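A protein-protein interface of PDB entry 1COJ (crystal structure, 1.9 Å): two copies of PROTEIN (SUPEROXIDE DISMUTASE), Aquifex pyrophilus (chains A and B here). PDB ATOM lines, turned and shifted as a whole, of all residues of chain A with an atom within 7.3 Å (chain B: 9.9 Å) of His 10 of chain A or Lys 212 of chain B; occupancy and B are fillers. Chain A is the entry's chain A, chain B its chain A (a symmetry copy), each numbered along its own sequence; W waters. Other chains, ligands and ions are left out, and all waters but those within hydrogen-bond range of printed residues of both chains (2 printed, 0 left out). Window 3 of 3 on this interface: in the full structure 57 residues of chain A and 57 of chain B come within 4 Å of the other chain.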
ATOM      1  N   PRO A   7      12.476 -31.895  -4.235  1.00  0.00           N
ATOM      2  CA  PRO A   7      13.718 -31.753  -3.473  1.00  0.00           C
ATOM      3  C   PRO A   7      13.918 -30.345  -2.922  1.00  0.00           C
ATOM      4  O   PRO A   7      13.392 -29.371  -3.468  1.00  0.00           O
ATOM      5  CB  PRO A   7      14.790 -32.134  -4.499  1.00  0.00           C
ATOM      6  CG  PRO A   7      14.180 -31.733  -5.798  1.00  0.00           C
ATOM      7  CD  PRO A   7      12.757 -32.203  -5.649  1.00  0.00           C
ATOM      8  N   LYS A   8      14.635 -30.249  -1.809  1.00  0.00           N
ATOM      9  CA  LYS A   8      14.916 -28.963  -1.196  1.00  0.00           C
ATOM     10  C   LYS A   8      16.361 -28.603  -1.501  1.00  0.00           C
ATOM     11  O   LYS A   8      17.260 -28.865  -0.701  1.00  0.00           O
ATOM     12  CB  LYS A   8      14.676 -29.033   0.310  1.00  0.00           C
ATOM     13  CG  LYS A   8      13.254 -29.422   0.660  1.00  0.00           C
ATOM     14  CD  LYS A   8      13.009 -29.369   2.147  1.00  0.00           C
ATOM     15  CE  LYS A   8      11.583 -29.770   2.454  1.00  0.00           C
ATOM     16  NZ  LYS A   8      11.282 -29.586   3.894  1.00  0.00           N
ATOM     17  N   ASP A   9      16.573 -28.000  -2.668  1.00  0.00           N
ATOM     18  CA  ASP A   9      17.908 -27.608  -3.114  1.00  0.00           C
ATOM     19  C   ASP A   9      18.661 -26.717  -2.146  1.00  0.00           C
ATOM     20  O   ASP A   9      19.877 -26.817  -2.031  1.00  0.00           O
ATOM     21  CB  ASP A   9      17.848 -26.942  -4.488  1.00  0.00           C
ATOM     22  CG  ASP A   9      17.594 -27.932  -5.598  1.00  0.00           C
ATOM     23  OD1 ASP A   9      18.529 -28.672  -5.971  1.00  0.00           O
ATOM     24  OD2 ASP A   9      16.455 -27.981  -6.088  1.00  0.00           O
ATOM     25  N   HIS A  10      17.938 -25.891  -1.400  1.00  0.00           N
ATOM     26  CA  HIS A  10      18.568 -24.987  -0.450  1.00  0.00           C
ATOM     27  C   HIS A  10      19.285 -25.707   0.697  1.00  0.00           C
ATOM     28  O   HIS A  10      19.983 -25.075   1.487  1.00  0.00           O
ATOM     29  CB  HIS A  10      17.540 -24.000   0.113  1.00  0.00           C
ATOM     30  CG  HIS A  10      16.583 -24.600   1.097  1.00  0.00           C
ATOM     31  ND1 HIS A  10      15.351 -25.102   0.745  1.00  0.00           N
ATOM     32  CD2 HIS A  10      16.670 -24.745   2.448  1.00  0.00           C
ATOM     33  CE1 HIS A  10      14.719 -25.526   1.820  1.00  0.00           C
ATOM     34  NE2 HIS A  10      15.495 -25.322   2.866  1.00  0.00           N
ATOM     35  N   LEU A  11      19.090 -27.018   0.790  1.00  0.00           N
ATOM     36  CA  LEU A  11      19.702 -27.836   1.836  1.00  0.00           C
ATOM     37  C   LEU A  11      21.081 -28.380   1.460  1.00  0.00           C
ATOM     38  O   LEU A  11      21.776 -28.937   2.307  1.00  0.00           O
ATOM     39  CB  LEU A  11      18.776 -29.015   2.161  1.00  0.00           C
ATOM     40  CG  LEU A  11      17.978 -29.052   3.465  1.00  0.00           C
ATOM     41  CD1 LEU A  11      17.509 -27.680   3.884  1.00  0.00           C
ATOM     42  CD2 LEU A  11      16.808 -30.009   3.300  1.00  0.00           C
ATOM     43  N   LYS A  12      21.464 -28.246   0.192  1.00  0.00           N
ATOM     44  CA  LYS A  12      22.748 -28.760  -0.287  1.00  0.00           C
ATOM     45  C   LYS A  12      23.966 -28.084   0.352  1.00  0.00           C
ATOM     46  O   LYS A  12      24.184 -26.882   0.178  1.00  0.00           O
ATOM     47  CB  LYS A  12      22.825 -28.629  -1.806  1.00  0.00           C
ATOM     48  CG  LYS A  12      23.982 -29.371  -2.438  1.00  0.00           C
ATOM     49  CD  LYS A  12      23.937 -29.196  -3.940  1.00  0.00           C
ATOM     50  CE  LYS A  12      25.075 -29.919  -4.624  1.00  0.00           C
ATOM     51  NZ  LYS A  12      25.034 -29.654  -6.083  1.00  0.00           N
ATOM     52  N   PRO A  13      24.785 -28.858   1.086  1.00  0.00           N
ATOM     53  CA  PRO A  13      25.988 -28.357   1.759  1.00  0.00           C
ATOM     54  C   PRO A  13      27.099 -28.136   0.738  1.00  0.00           C
ATOM     55  O   PRO A  13      27.123 -28.779  -0.316  1.00  0.00           O
ATOM     56  CB  PRO A  13      26.366 -29.505   2.706  1.00  0.00           C
ATOM     57  CG  PRO A  13      25.139 -30.368   2.771  1.00  0.00           C
ATOM     58  CD  PRO A  13      24.592 -30.285   1.386  1.00  0.00           C
ATOM     59  N   PHE A  28      23.673 -35.877  -3.082  1.00  0.00           N
ATOM     60  CA  PHE A  28      22.532 -34.973  -3.135  1.00  0.00           C
ATOM     61  C   PHE A  28      21.767 -35.036  -4.456  1.00  0.00           C
ATOM     62  O   PHE A  28      20.552 -35.234  -4.471  1.00  0.00           O
ATOM     63  CB  PHE A  28      22.987 -33.532  -2.879  1.00  0.00           C
ATOM     64  CG  PHE A  28      21.860 -32.582  -2.594  1.00  0.00           C
ATOM     65  CD1 PHE A  28      21.452 -32.343  -1.284  1.00  0.00           C
ATOM     66  CD2 PHE A  28      21.195 -31.938  -3.634  1.00  0.00           C
ATOM     67  CE1 PHE A  28      20.391 -31.474  -1.010  1.00  0.00           C
ATOM     68  CE2 PHE A  28      20.135 -31.070  -3.373  1.00  0.00           C
ATOM     69  CZ  PHE A  28      19.732 -30.837  -2.058  1.00  0.00           C
ATOM     70  N   GLU A  82      17.190 -35.193   4.223  1.00  0.00           N
ATOM     71  CA  GLU A  82      16.937 -33.781   4.482  1.00  0.00           C
ATOM     72  C   GLU A  82      17.419 -33.384   5.872  1.00  0.00           C
ATOM     73  O   GLU A  82      17.936 -32.281   6.064  1.00  0.00           O
ATOM     74  CB  GLU A  82      15.460 -33.452   4.291  1.00  0.00           C
ATOM     75  CG  GLU A  82      15.035 -33.577   2.845  1.00  0.00           C
ATOM     76  CD  GLU A  82      13.614 -33.125   2.588  1.00  0.00           C
ATOM     77  OE1 GLU A  82      13.259 -33.002   1.400  1.00  0.00           O
ATOM     78  OE2 GLU A  82      12.852 -32.899   3.552  1.00  0.00           O
ATOM     79  N   LEU A  83      17.274 -34.291   6.832  1.00  0.00           N
ATOM     80  CA  LEU A  83      17.722 -34.042   8.200  1.00  0.00           C
ATOM     81  C   LEU A  83      19.252 -34.060   8.266  1.00  0.00           C
ATOM     82  O   LEU A  83      19.867 -33.329   9.044  1.00  0.00           O
ATOM     83  CB  LEU A  83      17.146 -35.103   9.144  1.00  0.00           C
ATOM     84  CG  LEU A  83      15.635 -35.069   9.401  1.00  0.00           C
ATOM     85  CD1 LEU A  83      15.191 -36.354  10.072  1.00  0.00           C
ATOM     86  CD2 LEU A  83      15.283 -33.868  10.265  1.00  0.00           C
ATOM     87  N   PHE A  85      21.603 -33.480   5.492  1.00  0.00           N
ATOM     88  CA  PHE A  85      22.177 -32.325   4.807  1.00  0.00           C
ATOM     89  C   PHE A  85      21.872 -31.022   5.537  1.00  0.00           C
ATOM     90  O   PHE A  85      22.744 -30.162   5.686  1.00  0.00           O
ATOM     91  CB  PHE A  85      21.650 -32.239   3.373  1.00  0.00           C
ATOM     92  CG  PHE A  85      22.120 -33.352   2.480  1.00  0.00           C
ATOM     93  CD1 PHE A  85      23.476 -33.639   2.359  1.00  0.00           C
ATOM     94  CD2 PHE A  85      21.206 -34.105   1.745  1.00  0.00           C
ATOM     95  CE1 PHE A  85      23.918 -34.654   1.522  1.00  0.00           C
ATOM     96  CE2 PHE A  85      21.639 -35.125   0.903  1.00  0.00           C
ATOM     97  CZ  PHE A  85      22.997 -35.399   0.790  1.00  0.00           C
ATOM     98  N   GLY A  86      20.641 -30.904   6.027  1.00  0.00           N
ATOM     99  CA  GLY A  86      20.211 -29.709   6.729  1.00  0.00           C
ATOM    100  C   GLY A  86      20.963 -29.342   7.991  1.00  0.00           C
ATOM    101  O   GLY A  86      20.909 -28.195   8.436  1.00  0.00           O
ATOM    102  N   GLU A 195      17.447 -26.293  17.883  1.00  0.00           N
ATOM    103  CA  GLU A 195      16.066 -25.967  17.559  1.00  0.00           C
ATOM    104  C   GLU A 195      15.228 -27.236  17.520  1.00  0.00           C
ATOM    105  O   GLU A 195      14.103 -27.259  18.020  1.00  0.00           O
ATOM    106  CB  GLU A 195      15.964 -25.244  16.219  1.00  0.00           C
ATOM    107  CG  GLU A 195      14.522 -25.051  15.776  1.00  0.00           C
ATOM    108  CD  GLU A 195      14.374 -24.121  14.595  1.00  0.00           C
ATOM    109  OE1 GLU A 195      13.496 -23.235  14.661  1.00  0.00           O
ATOM    110  OE2 GLU A 195      15.121 -24.274  13.604  1.00  0.00           O
ATOM    111  N   ARG A 196      15.779 -28.285  16.917  1.00  0.00           N
ATOM    112  CA  ARG A 196      15.089 -29.565  16.834  1.00  0.00           C
ATOM    113  C   ARG A 196      14.774 -30.051  18.246  1.00  0.00           C
ATOM    114  O   ARG A 196      13.665 -30.513  18.520  1.00  0.00           O
ATOM    115  CB  ARG A 196      15.954 -30.602  16.118  1.00  0.00           C
ATOM    116  CG  ARG A 196      16.163 -30.339  14.638  1.00  0.00           C
ATOM    117  CD  ARG A 196      16.997 -31.441  14.007  1.00  0.00           C
ATOM    118  NE  ARG A 196      17.273 -31.186  12.594  1.00  0.00           N
ATOM    119  CZ  ARG A 196      18.183 -31.840  11.878  1.00  0.00           C
ATOM    120  NH1 ARG A 196      18.911 -32.797  12.430  1.00  0.00           N
ATOM    121  NH2 ARG A 196      18.400 -31.501  10.615  1.00  0.00           N
ATOM    122  N   LYS A 199      11.861 -28.095  19.963  1.00  0.00           N
ATOM    123  CA  LYS A 199      10.589 -28.542  19.411  1.00  0.00           C
ATOM    124  C   LYS A 199      10.242 -29.937  19.913  1.00  0.00           C
ATOM    125  O   LYS A 199       9.096 -30.207  20.276  1.00  0.00           O
ATOM    126  CB  LYS A 199      10.643 -28.531  17.884  1.00  0.00           C
ATOM    127  CG  LYS A 199      10.837 -27.150  17.289  1.00  0.00           C
ATOM    128  CD  LYS A 199      10.754 -27.182  15.778  1.00  0.00           C
ATOM    129  CE  LYS A 199      10.754 -25.774  15.215  1.00  0.00           C
ATOM    130  NZ  LYS A 199      10.550 -25.744  13.741  1.00  0.00           N
ATOM    131  N   PHE B 136       6.425 -35.279  10.039  1.00  0.00           N
ATOM    132  CA  PHE B 136       7.140 -34.547   9.001  1.00  0.00           C
ATOM    133  C   PHE B 136       6.230 -33.868   7.986  1.00  0.00           C
ATOM    134  O   PHE B 136       6.614 -32.854   7.401  1.00  0.00           O
ATOM    135  CB  PHE B 136       8.163 -35.450   8.311  1.00  0.00           C
ATOM    136  CG  PHE B 136       9.174 -36.047   9.258  1.00  0.00           C
ATOM    137  CD1 PHE B 136      10.103 -35.240   9.915  1.00  0.00           C
ATOM    138  CD2 PHE B 136       9.175 -37.414   9.517  1.00  0.00           C
ATOM    139  CE1 PHE B 136      11.014 -35.787  10.815  1.00  0.00           C
ATOM    140  CE2 PHE B 136      10.082 -37.968  10.415  1.00  0.00           C
ATOM    141  CZ  PHE B 136      11.002 -37.152  11.066  1.00  0.00           C
ATOM    142  N   ALA B 206       3.973 -28.086  17.825  1.00  0.00           N
ATOM    143  CA  ALA B 206       5.322 -27.732  18.275  1.00  0.00           C
ATOM    144  C   ALA B 206       6.374 -28.236  17.284  1.00  0.00           C
ATOM    145  O   ALA B 206       7.480 -27.704  17.215  1.00  0.00           O
ATOM    146  CB  ALA B 206       5.588 -28.322  19.655  1.00  0.00           C
ATOM    147  N   LEU B 207       6.003 -29.251  16.508  1.00  0.00           N
ATOM    148  CA  LEU B 207       6.879 -29.883  15.526  1.00  0.00           C
ATOM    149  C   LEU B 207       6.752 -29.391  14.085  1.00  0.00           C
ATOM    150  O   LEU B 207       7.556 -29.781  13.234  1.00  0.00           O
ATOM    151  CB  LEU B 207       6.639 -31.396  15.545  1.00  0.00           C
ATOM    152  CG  LEU B 207       7.658 -32.377  16.130  1.00  0.00           C
ATOM    153  CD1 LEU B 207       8.510 -31.743  17.206  1.00  0.00           C
ATOM    154  CD2 LEU B 207       6.907 -33.582  16.666  1.00  0.00           C
ATOM    155  N   LYS B 208       5.744 -28.581  13.775  1.00  0.00           N
ATOM    156  CA  LYS B 208       5.596 -28.127  12.396  1.00  0.00           C
ATOM    157  C   LYS B 208       6.829 -27.390  11.903  1.00  0.00           C
ATOM    158  O   LYS B 208       7.477 -26.666  12.658  1.00  0.00           O
ATOM    159  CB  LYS B 208       4.326 -27.298  12.181  1.00  0.00           C
ATOM    160  CG  LYS B 208       4.287 -25.933  12.815  1.00  0.00           C
ATOM    161  CD  LYS B 208       3.005 -25.255  12.378  1.00  0.00           C
ATOM    162  CE  LYS B 208       2.650 -24.084  13.261  1.00  0.00           C
ATOM    163  NZ  LYS B 208       1.185 -23.823  13.189  1.00  0.00           N
ATOM    164  N   ASP B 209       7.160 -27.617  10.636  1.00  0.00           N
ATOM    165  CA  ASP B 209       8.332 -27.016  10.003  1.00  0.00           C
ATOM    166  C   ASP B 209       9.613 -27.536  10.654  1.00  0.00           C
ATOM    167  O   ASP B 209      10.588 -26.799  10.806  1.00  0.00           O
ATOM    168  CB  ASP B 209       8.281 -25.481  10.077  1.00  0.00           C
ATOM    169  CG  ASP B 209       7.132 -24.892   9.277  1.00  0.00           C
ATOM    170  OD1 ASP B 209       6.338 -24.119   9.859  1.00  0.00           O
ATOM    171  OD2 ASP B 209       7.027 -25.197   8.068  1.00  0.00           O
ATOM    172  N   PHE B 210       9.599 -28.814  11.029  1.00  0.00           N
ATOM    173  CA  PHE B 210      10.751 -29.454  11.663  1.00  0.00           C
ATOM    174  C   PHE B 210      11.936 -29.396  10.699  1.00  0.00           C
ATOM    175  O   PHE B 210      13.069 -29.115  11.095  1.00  0.00           O
ATOM    176  CB  PHE B 210      10.413 -30.904  12.014  1.00  0.00           C
ATOM    177  CG  PHE B 210      11.376 -31.533  12.972  1.00  0.00           C
ATOM    178  CD1 PHE B 210      11.342 -31.208  14.319  1.00  0.00           C
ATOM    179  CD2 PHE B 210      12.317 -32.454  12.527  1.00  0.00           C
ATOM    180  CE1 PHE B 210      12.236 -31.790  15.212  1.00  0.00           C
ATOM    181  CE2 PHE B 210      13.213 -33.038  13.410  1.00  0.00           C
ATOM    182  CZ  PHE B 210      13.174 -32.708  14.754  1.00  0.00           C
ATOM    183  N   ILE B 211      11.667 -29.711   9.437  1.00  0.00           N
ATOM    184  CA  ILE B 211      12.686 -29.644   8.400  1.00  0.00           C
ATOM    185  C   ILE B 211      12.366 -28.338   7.671  1.00  0.00           C
ATOM    186  O   ILE B 211      11.232 -28.130   7.234  1.00  0.00           O
ATOM    187  CB  ILE B 211      12.581 -30.820   7.401  1.00  0.00           C
ATOM    188  CG1 ILE B 211      12.668 -32.155   8.140  1.00  0.00           C
ATOM    189  CG2 ILE B 211      13.700 -30.724   6.366  1.00  0.00           C
ATOM    190  CD1 ILE B 211      12.405 -33.356   7.259  1.00  0.00           C
ATOM    191  N   LYS B 212      13.340 -27.443   7.589  1.00  0.00           N
ATOM    192  CA  LYS B 212      13.138 -26.160   6.931  1.00  0.00           C
ATOM    193  C   LYS B 212      13.962 -26.027   5.652  1.00  0.00           C
ATOM    194  O   LYS B 212      15.201 -26.139   5.724  1.00  0.00           O
ATOM    195  CB  LYS B 212      13.463 -25.024   7.907  1.00  0.00           C
ATOM    196  CG  LYS B 212      12.654 -25.091   9.198  1.00  0.00           C
ATOM    197  CD  LYS B 212      12.946 -23.931  10.133  1.00  0.00           C
ATOM    198  CE  LYS B 212      12.026 -23.981  11.343  1.00  0.00           C
ATOM    199  NZ  LYS B 212      12.197 -22.805  12.243  1.00  0.00           N
ATOM    200  OXT LYS B 212      13.362 -25.822   4.579  1.00  0.00           O
HETATM  201  O   HOH W   1      15.706 -29.175  10.973  1.00  0.00           O
HETATM  202  O   HOH W   2      13.328 -27.162  13.045  1.00  0.00           O
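His 10 of chain A touches one residue of chain B.
Lys 212 of chain B touches just these residues of chain A: His 10, Leu 11, Glu 195 and Lys 199.
Lys 8 of chain A touches one residue of chain B.
Leu 11 of chain A touches just one residue of chain B: Lys 212.
Printed residues of chain B within 4 Å of Glu 82 of chain A: Ile 211.
Of the printed residues of chain B, Arg 196 of chain A touches Phe 210.
Printed residues of chain A within 4 Å of Lys 208 of chain B: Lys 199 (3.4 Å).
Phe 85 of chain A touches none of the printed residues of chain B.
Pro 13 of chain A touches none of the printed residues of chain B.
The nearest residue of chain B that does not touch His 10 of chain A is Ile 211 of chain B (6.5 Å).
The nearest residue of chain A that does not touch Lys 212 of chain B is Lys 8 of chain A (4.3 Å).
The nearest printed residue of chain A that does not touch Phe 210 of chain B is Lys 199 of chain A (4.2 Å).
Water W1 lies within hydrogen-bond range of O of Phe 210 of chain B and NE of Arg 196 of chain A.
Water W2 lies within hydrogen-bond range of the backbone carbonyl oxygen of Phe 210 of chain B (2.8 Å), the side-chain amino group of Lys 199 of chain A (3.2 Å) and the side-chain carboxylate of Glu 195 of chain A (3.4 Å).
Hydrophobic or aromatic side chains of chain B that line the printed part of chain A: Leu 207, Phe 210 and Ile 211.
Along chain B the printed residues that touch a printed residue of chain A span positions 206 to 212.
Among the printed residues, Asp or Glu carboxylates within 4 Å of a Lys or Arg side-chain nitrogen of the other chain: Glu 195 of chain A with Lys 212 of chain B (2.8 Å).
The side-chain carboxylate (OE1) of Glu 195 of chain A lies within salt-bridge range of the side-chain amino group (NZ) of Lys 212 of chain B (2.8 Å).
O of Asp 209 of chain B is in hydrogen-bond range of NZ of Lys 199 of chain A (3.1 Å).
NE2 of His 10 of chain A is in hydrogen-bond range of OXT of Lys 212 of chain B.
The backbone carbonyl oxygen (O) of Lys 208 of chain B is in hydrogen-bond range of the side-chain amino group (NZ) of Lys 199 of chain A (3.4 Å).
Among the printed residues, merely in contact across the chains: Lys 8 of chain A with Ile 211 of chain B (3.6 Å), Leu 11 of chain A with Lys 212 of chain B (3.3 Å), Glu 82 of chain A with Ile 211 of chain B (3.7 Å), Leu 83 of chain A with Phe 210 of chain B (3.9 Å), Leu 83 of chain A with Ile 211 of chain B (3.8 Å), Arg 196 of chain A with Phe 210 of chain B (3.7 Å), Lys 199 of chain A with Ala 206 of chain B (3.3 Å), Lys 199 of chain A with Leu 207 of chain B (3.5 Å) and Lys 199 of chain A with Lys 212 of chain B (3.3 Å).
No position is printed for both chains.
The side-chain carboxylate of Glu 195 of chain A lies within salt-bridge range of the side-chain amino group of Lys 199 of chain A (3.98 Å).
The side-chain carboxylate (OE2) of Glu 82 of chain A is in salt-bridge range of the side-chain amino group (NZ) of Lys 8 of chain A, 3.7 Å away.
The backbone carbonyl oxygen of Leu 83 of chain A is in hydrogen-bond range of the guanidinium group of Arg 196 of chain A.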
